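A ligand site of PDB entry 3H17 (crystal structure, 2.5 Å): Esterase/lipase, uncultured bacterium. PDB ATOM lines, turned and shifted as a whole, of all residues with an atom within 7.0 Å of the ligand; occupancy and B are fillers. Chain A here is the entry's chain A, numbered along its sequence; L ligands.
N of Ala 158 is in hydrogen-bond range of O2 of the ligand (3.3 Å).
The backbone NH of Gly 89 sits at hydrogen-bond distance from an oxygen (O2) of the ligand (3.0 Å).
The backbone NH (N) of Gly 90 sits at hydrogen-bond distance from an oxygen (O2) of the ligand, 2.8 Å away.
S1 of the ligand is covalently linked to OG of Ser 157 (1.8 Å).
The side-chain carboxylate (OE1) of Glu 251 sits at hydrogen-bond distance from a ring nitrogen (ND1) of His 281.
OG of Ser 157 sits at hydrogen-bond distance from NE2 of His 281, at 3.0 Å.
N of Gly 88 sits at hydrogen-bond distance from NE2 of His 99, 3.2 Å away.
O of Ser 157 is in hydrogen-bond range of N of Trp 187.
O of Ala 158 is in hydrogen-bond range of OH of Tyr 91.
The backbone NH (N) of Gly 88 sits at hydrogen-bond distance from the side-chain carboxylate (OD1) of Asp 156.
The backbone NH (N) of Ser 157 sits close to the backbone carbonyl oxygen (O) of Ser 185, 3.3 Å away.
Gly 88 touches the ligand (C to O2, 3.97 Å).
Met 93 touches the ligand.
Trp 187 touches the ligand.
CE of Met 215 touches C4 of the ligand, 3.6 Å away.
His 281 touches the ligand.
Hydrophobic or aromatic side chains that line the ligand: Met 93, Ala 158, Trp 187, Met 215 and His 281.
The nearest printed residue that does not touch the ligand is Ile 212 (4.03 Å).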
ATOM      1  N   MET A  42     -15.210  -2.248  28.735  1.00  0.00           N
ATOM      2  CA  MET A  42     -14.639  -1.007  28.199  1.00  0.00           C
ATOM      3  C   MET A  42     -13.074  -0.951  28.173  1.00  0.00           C
ATOM      4  O   MET A  42     -12.490  -0.521  27.152  1.00  0.00           O
ATOM      5  CB  MET A  42     -15.190   0.173  28.961  1.00  0.00           C
ATOM      6  CG  MET A  42     -16.499   0.736  28.412  1.00  0.00           C
ATOM      7  SD  MET A  42     -16.975   2.179  29.410  1.00  0.00           S
ATOM      8  CE  MET A  42     -17.153   1.575  31.137  1.00  0.00           C
ATOM      9  N   MET A  46     -10.311  -0.802  24.892  1.00  0.00           N
ATOM     10  CA  MET A  46      -9.323   0.199  24.634  1.00  0.00           C
ATOM     11  C   MET A  46      -7.949  -0.428  24.435  1.00  0.00           C
ATOM     12  O   MET A  46      -7.173   0.046  23.609  1.00  0.00           O
ATOM     13  CB  MET A  46      -9.313   1.134  25.780  1.00  0.00           C
ATOM     14  CG  MET A  46      -9.795   2.494  25.477  1.00  0.00           C
ATOM     15  SD  MET A  46      -8.994   3.549  26.715  1.00  0.00           S
ATOM     16  CE  MET A  46      -9.053   5.072  25.779  1.00  0.00           C
ATOM     17  N   HIS A  87      -2.420  10.233  30.487  1.00  0.00           N
ATOM     18  CA  HIS A  87      -3.335   9.753  29.469  1.00  0.00           C
ATOM     19  C   HIS A  87      -4.748  10.008  29.864  1.00  0.00           C
ATOM     20  O   HIS A  87      -5.111  10.005  31.035  1.00  0.00           O
ATOM     21  CB  HIS A  87      -3.199   8.220  29.274  1.00  0.00           C
ATOM     22  CG  HIS A  87      -3.414   7.419  30.510  1.00  0.00           C
ATOM     23  ND1 HIS A  87      -4.671   7.054  30.944  1.00  0.00           N
ATOM     24  CD2 HIS A  87      -2.526   6.907  31.411  1.00  0.00           C
ATOM     25  CE1 HIS A  87      -4.557   6.300  32.039  1.00  0.00           C
ATOM     26  NE2 HIS A  87      -3.274   6.261  32.397  1.00  0.00           N
ATOM     27  N   GLY A  88      -5.605  10.157  28.863  1.00  0.00           N
ATOM     28  CA  GLY A  88      -7.040  10.228  29.172  1.00  0.00           C
ATOM     29  C   GLY A  88      -7.562   8.809  29.339  1.00  0.00           C
ATOM     30  O   GLY A  88      -6.717   7.831  29.309  1.00  0.00           O
ATOM     31  N   GLY A  89      -8.918   8.742  29.506  1.00  0.00           N
ATOM     32  CA  GLY A  89      -9.708   7.603  29.731  1.00  0.00           C
ATOM     33  C   GLY A  89     -10.683   7.842  30.897  1.00  0.00           C
ATOM     34  O   GLY A  89     -11.040   6.901  31.677  1.00  0.00           O
ATOM     35  N   GLY A  90     -11.118   9.034  31.147  1.00  0.00           N
ATOM     36  CA  GLY A  90     -12.334   8.973  31.987  1.00  0.00           C
ATOM     37  C   GLY A  90     -11.996   8.847  33.474  1.00  0.00           C
ATOM     38  O   GLY A  90     -12.932   8.918  34.386  1.00  0.00           O
ATOM     39  N   TYR A  91     -10.694   8.740  33.743  1.00  0.00           N
ATOM     40  CA  TYR A  91     -10.132   8.370  35.067  1.00  0.00           C
ATOM     41  C   TYR A  91     -10.373   6.939  35.513  1.00  0.00           C
ATOM     42  O   TYR A  91      -9.908   6.586  36.622  1.00  0.00           O
ATOM     43  CB  TYR A  91     -10.571   9.292  36.234  1.00  0.00           C
ATOM     44  CG  TYR A  91     -10.070  10.747  36.204  1.00  0.00           C
ATOM     45  CD1 TYR A  91     -10.877  11.781  35.747  1.00  0.00           C
ATOM     46  CD2 TYR A  91      -8.782  11.083  36.560  1.00  0.00           C
ATOM     47  CE1 TYR A  91     -10.452  13.133  35.701  1.00  0.00           C
ATOM     48  CE2 TYR A  91      -8.370  12.473  36.535  1.00  0.00           C
ATOM     49  CZ  TYR A  91      -9.226  13.448  36.104  1.00  0.00           C
ATOM     50  OH  TYR A  91      -8.865  14.795  36.052  1.00  0.00           O
ATOM     51  N   VAL A  92     -11.006   6.122  34.694  1.00  0.00           N
ATOM     52  CA  VAL A  92     -11.388   4.782  35.053  1.00  0.00           C
ATOM     53  C   VAL A  92     -10.731   3.814  34.119  1.00  0.00           C
ATOM     54  O   VAL A  92     -10.813   2.639  34.293  1.00  0.00           O
ATOM     55  CB  VAL A  92     -12.915   4.577  34.981  1.00  0.00           C
ATOM     56  CG1 VAL A  92     -13.626   5.439  35.935  1.00  0.00           C
ATOM     57  CG2 VAL A  92     -13.420   4.814  33.614  1.00  0.00           C
ATOM     58  N   MET A  93     -10.073   4.331  33.109  1.00  0.00           N
ATOM     59  CA  MET A  93      -9.414   3.511  32.087  1.00  0.00           C
ATOM     60  C   MET A  93      -8.169   4.083  31.311  1.00  0.00           C
ATOM     61  O   MET A  93      -7.674   5.225  31.620  1.00  0.00           O
ATOM     62  CB  MET A  93     -10.480   3.046  31.137  1.00  0.00           C
ATOM     63  CG  MET A  93     -11.013   4.091  30.217  1.00  0.00           C
ATOM     64  SD  MET A  93     -12.315   3.147  29.351  1.00  0.00           S
ATOM     65  CE  MET A  93     -12.747   4.250  28.002  1.00  0.00           C
ATOM     66  N   HIS A  99      -1.752   4.665  25.181  1.00  0.00           N
ATOM     67  CA  HIS A  99      -1.401   5.989  24.773  1.00  0.00           C
ATOM     68  C   HIS A  99       0.067   6.099  24.298  1.00  0.00           C
ATOM     69  O   HIS A  99       0.528   7.195  23.941  1.00  0.00           O
ATOM     70  CB  HIS A  99      -1.690   6.962  25.900  1.00  0.00           C
ATOM     71  CG  HIS A  99      -3.126   7.415  25.988  1.00  0.00           C
ATOM     72  ND1 HIS A  99      -4.202   6.553  26.269  1.00  0.00           N
ATOM     73  CD2 HIS A  99      -3.657   8.671  25.934  1.00  0.00           C
ATOM     74  CE1 HIS A  99      -5.316   7.269  26.298  1.00  0.00           C
ATOM     75  NE2 HIS A  99      -5.022   8.552  26.100  1.00  0.00           N
ATOM     76  N   TYR A 119      -0.994   6.076  36.265  1.00  0.00           N
ATOM     77  CA  TYR A 119      -1.459   6.512  37.570  1.00  0.00           C
ATOM     78  C   TYR A 119      -2.698   5.734  37.977  1.00  0.00           C
ATOM     79  O   TYR A 119      -3.378   5.080  37.099  1.00  0.00           O
ATOM     80  CB  TYR A 119      -1.836   8.020  37.458  1.00  0.00           C
ATOM     81  CG  TYR A 119      -2.909   8.360  36.412  1.00  0.00           C
ATOM     82  CD1 TYR A 119      -4.303   8.184  36.701  1.00  0.00           C
ATOM     83  CD2 TYR A 119      -2.560   8.807  35.106  1.00  0.00           C
ATOM     84  CE1 TYR A 119      -5.314   8.478  35.765  1.00  0.00           C
ATOM     85  CE2 TYR A 119      -3.595   9.156  34.106  1.00  0.00           C
ATOM     86  CZ  TYR A 119      -4.960   9.005  34.454  1.00  0.00           C
ATOM     87  OH  TYR A 119      -6.000   9.340  33.524  1.00  0.00           O
ATOM     88  N   ASP A 156      -4.174  14.159  27.706  1.00  0.00           N
ATOM     89  CA  ASP A 156      -5.468  14.248  26.993  1.00  0.00           C
ATOM     90  C   ASP A 156      -6.696  13.919  27.890  1.00  0.00           C
ATOM     91  O   ASP A 156      -6.774  12.925  28.633  1.00  0.00           O
ATOM     92  CB  ASP A 156      -5.539  13.339  25.805  1.00  0.00           C
ATOM     93  CG  ASP A 156      -5.136  11.916  26.180  1.00  0.00           C
ATOM     94  OD1 ASP A 156      -5.971  11.011  26.012  1.00  0.00           O
ATOM     95  OD2 ASP A 156      -3.998  11.728  26.753  1.00  0.00           O
ATOM     96  N   SER A 157      -7.694  14.744  27.735  1.00  0.00           N
ATOM     97  CA  SER A 157      -8.986  14.339  28.180  1.00  0.00           C
ATOM     98  C   SER A 157      -9.041  14.364  29.686  1.00  0.00           C
ATOM     99  O   SER A 157      -8.883  15.442  30.332  1.00  0.00           O
ATOM    100  CB  SER A 157      -9.170  12.945  27.777  1.00  0.00           C
ATOM    101  OG  SER A 157     -10.557  12.863  27.636  1.00  0.00           O
ATOM    102  N   ALA A 158      -9.244  13.181  30.299  1.00  0.00           N
ATOM    103  CA  ALA A 158      -9.227  13.244  31.734  1.00  0.00           C
ATOM    104  C   ALA A 158      -7.815  13.649  32.087  1.00  0.00           C
ATOM    105  O   ALA A 158      -7.612  14.388  33.048  1.00  0.00           O
ATOM    106  CB  ALA A 158      -9.569  11.958  32.272  1.00  0.00           C
ATOM    107  N   GLY A 159      -6.838  13.236  31.223  1.00  0.00           N
ATOM    108  CA  GLY A 159      -5.440  13.411  31.474  1.00  0.00           C
ATOM    109  C   GLY A 159      -5.321  14.925  31.412  1.00  0.00           C
ATOM    110  O   GLY A 159      -4.539  15.550  32.161  1.00  0.00           O
ATOM    111  N   GLY A 160      -6.063  15.549  30.492  1.00  0.00           N
ATOM    112  CA  GLY A 160      -5.835  16.981  30.350  1.00  0.00           C
ATOM    113  C   GLY A 160      -6.275  17.749  31.580  1.00  0.00           C
ATOM    114  O   GLY A 160      -5.642  18.822  31.946  1.00  0.00           O
ATOM    115  N   SER A 185      -7.839  18.434  24.575  1.00  0.00           N
ATOM    116  CA  SER A 185      -9.248  18.133  24.840  1.00  0.00           C
ATOM    117  C   SER A 185      -9.496  17.822  26.357  1.00  0.00           C
ATOM    118  O   SER A 185     -10.064  16.818  26.641  1.00  0.00           O
ATOM    119  CB  SER A 185      -9.710  16.889  24.060  1.00  0.00           C
ATOM    120  OG  SER A 185      -9.761  17.037  22.640  1.00  0.00           O
ATOM    121  N   PRO A 186      -9.125  18.723  27.305  1.00  0.00           N
ATOM    122  CA  PRO A 186      -9.166  18.378  28.725  1.00  0.00           C
ATOM    123  C   PRO A 186     -10.604  18.336  29.183  1.00  0.00           C
ATOM    124  O   PRO A 186     -11.429  19.117  28.721  1.00  0.00           O
ATOM    125  CB  PRO A 186      -8.543  19.611  29.416  1.00  0.00           C
ATOM    126  CG  PRO A 186      -8.931  20.782  28.436  1.00  0.00           C
ATOM    127  CD  PRO A 186      -8.777  20.142  27.090  1.00  0.00           C
ATOM    128  N   TRP A 187     -10.903  17.451  30.106  1.00  0.00           N
ATOM    129  CA  TRP A 187     -12.135  17.440  30.791  1.00  0.00           C
ATOM    130  C   TRP A 187     -11.842  18.101  32.126  1.00  0.00           C
ATOM    131  O   TRP A 187     -11.358  17.446  33.051  1.00  0.00           O
ATOM    132  CB  TRP A 187     -12.503  15.993  31.028  1.00  0.00           C
ATOM    133  CG  TRP A 187     -13.724  15.755  31.768  1.00  0.00           C
ATOM    134  CD1 TRP A 187     -14.832  16.635  31.937  1.00  0.00           C
ATOM    135  CD2 TRP A 187     -14.067  14.531  32.423  1.00  0.00           C
ATOM    136  NE1 TRP A 187     -15.815  15.990  32.729  1.00  0.00           N
ATOM    137  CE2 TRP A 187     -15.381  14.716  33.023  1.00  0.00           C
ATOM    138  CE3 TRP A 187     -13.389  13.286  32.587  1.00  0.00           C
ATOM    139  CZ2 TRP A 187     -16.021  13.687  33.769  1.00  0.00           C
ATOM    140  CZ3 TRP A 187     -14.026  12.270  33.351  1.00  0.00           C
ATOM    141  CH2 TRP A 187     -15.362  12.492  33.904  1.00  0.00           C
ATOM    142  N   GLY A 211     -22.605   8.302  29.656  1.00  0.00           N
ATOM    143  CA  GLY A 211     -21.557   7.373  30.059  1.00  0.00           C
ATOM    144  C   GLY A 211     -20.378   8.143  30.628  1.00  0.00           C
ATOM    145  O   GLY A 211     -19.633   7.620  31.477  1.00  0.00           O
ATOM    146  N   ILE A 212     -20.180   9.377  30.151  1.00  0.00           N
ATOM    147  CA  ILE A 212     -19.227  10.300  30.803  1.00  0.00           C
ATOM    148  C   ILE A 212     -19.674  10.719  32.213  1.00  0.00           C
ATOM    149  O   ILE A 212     -18.851  11.029  33.061  1.00  0.00           O
ATOM    150  CB  ILE A 212     -18.925  11.593  29.993  1.00  0.00           C
ATOM    151  CG1 ILE A 212     -17.757  12.347  30.661  1.00  0.00           C
ATOM    152  CG2 ILE A 212     -20.267  12.432  29.747  1.00  0.00           C
ATOM    153  CD1 ILE A 212     -16.923  13.322  29.747  1.00  0.00           C
ATOM    154  N   MET A 215     -18.615   7.860  34.737  1.00  0.00           N
ATOM    155  CA  MET A 215     -17.217   8.054  35.106  1.00  0.00           C
ATOM    156  C   MET A 215     -16.842   9.141  36.127  1.00  0.00           C
ATOM    157  O   MET A 215     -15.946   8.962  36.940  1.00  0.00           O
ATOM    158  CB  MET A 215     -16.418   8.242  33.841  1.00  0.00           C
ATOM    159  CG  MET A 215     -16.593   7.045  33.011  1.00  0.00           C
ATOM    160  SD  MET A 215     -15.559   7.348  31.643  1.00  0.00           S
ATOM    161  CE  MET A 215     -16.668   6.532  30.464  1.00  0.00           C
ATOM    162  N   GLU A 251     -16.694  18.424  19.281  1.00  0.00           N
ATOM    163  CA  GLU A 251     -16.652  17.606  20.432  1.00  0.00           C
ATOM    164  C   GLU A 251     -17.423  18.112  21.602  1.00  0.00           C
ATOM    165  O   GLU A 251     -17.657  19.291  21.852  1.00  0.00           O
ATOM    166  CB  GLU A 251     -15.223  17.201  20.790  1.00  0.00           C
ATOM    167  CG  GLU A 251     -14.288  18.185  21.336  1.00  0.00           C
ATOM    168  CD  GLU A 251     -12.992  17.491  21.799  1.00  0.00           C
ATOM    169  OE1 GLU A 251     -13.049  16.761  22.824  1.00  0.00           O
ATOM    170  OE2 GLU A 251     -11.925  17.655  21.158  1.00  0.00           O
ATOM    171  N   LEU A 253     -16.723  18.244  24.436  1.00  0.00           N
ATOM    172  CA  LEU A 253     -16.070  18.696  25.608  1.00  0.00           C
ATOM    173  C   LEU A 253     -15.617  20.094  25.295  1.00  0.00           C
ATOM    174  O   LEU A 253     -14.731  20.626  25.982  1.00  0.00           O
ATOM    175  CB  LEU A 253     -14.852  17.784  25.908  1.00  0.00           C
ATOM    176  CG  LEU A 253     -14.872  16.577  26.842  1.00  0.00           C
ATOM    177  CD1 LEU A 253     -13.460  16.205  26.966  1.00  0.00           C
ATOM    178  CD2 LEU A 253     -15.376  16.950  28.217  1.00  0.00           C
ATOM    179  N   HIS A 281     -12.639  14.696  19.409  1.00  0.00           N
ATOM    180  CA  HIS A 281     -11.934  14.403  20.590  1.00  0.00           C
ATOM    181  C   HIS A 281     -10.518  13.851  20.339  1.00  0.00           C
ATOM    182  O   HIS A 281     -10.351  12.824  19.702  1.00  0.00           O
ATOM    183  CB  HIS A 281     -12.747  13.454  21.446  1.00  0.00           C
ATOM    184  CG  HIS A 281     -12.174  13.267  22.827  1.00  0.00           C
ATOM    185  ND1 HIS A 281     -12.036  14.317  23.716  1.00  0.00           N
ATOM    186  CD2 HIS A 281     -11.730  12.162  23.478  1.00  0.00           C
ATOM    187  CE1 HIS A 281     -11.527  13.872  24.839  1.00  0.00           C
ATOM    188  NE2 HIS A 281     -11.283  12.575  24.708  1.00  0.00           N
ATOM    189  N   VAL A 282      -9.507  14.506  20.869  1.00  0.00           N
ATOM    190  CA  VAL A 282      -8.178  13.948  20.811  1.00  0.00           C
ATOM    191  C   VAL A 282      -7.790  13.395  19.397  1.00  0.00           C
ATOM    192  O   VAL A 282      -7.340  12.241  19.210  1.00  0.00           O
ATOM    193  CB  VAL A 282      -7.938  12.909  21.954  1.00  0.00           C
ATOM    194  CG1 VAL A 282      -6.449  12.849  22.174  1.00  0.00           C
ATOM    195  CG2 VAL A 282      -8.592  13.351  23.280  1.00  0.00           C
HETATM  196  C1  LIG L   1     -12.495  11.539  27.266  1.00  0.00           C
HETATM  197  S1  LIG L   1     -11.778  12.101  28.656  1.00  0.00           S
HETATM  198  C2  LIG L   1     -12.939  10.128  27.516  1.00  0.00           C
HETATM  199  C3  LIG L   1     -14.212   9.908  28.085  1.00  0.00           C
HETATM  200  C4  LIG L   1     -14.616   8.552  28.292  1.00  0.00           C
HETATM  201  C5  LIG L   1     -13.758   7.444  27.902  1.00  0.00           C
HETATM  202  C6  LIG L   1     -12.467   7.695  27.298  1.00  0.00           C
HETATM  203  C7  LIG L   1     -12.068   9.049  27.120  1.00  0.00           C
HETATM  204  O1  LIG L   1     -13.240  11.689  29.570  1.00  0.00           O
HETATM  205  O2  LIG L   1     -11.006  10.729  28.874  1.00  0.00           O
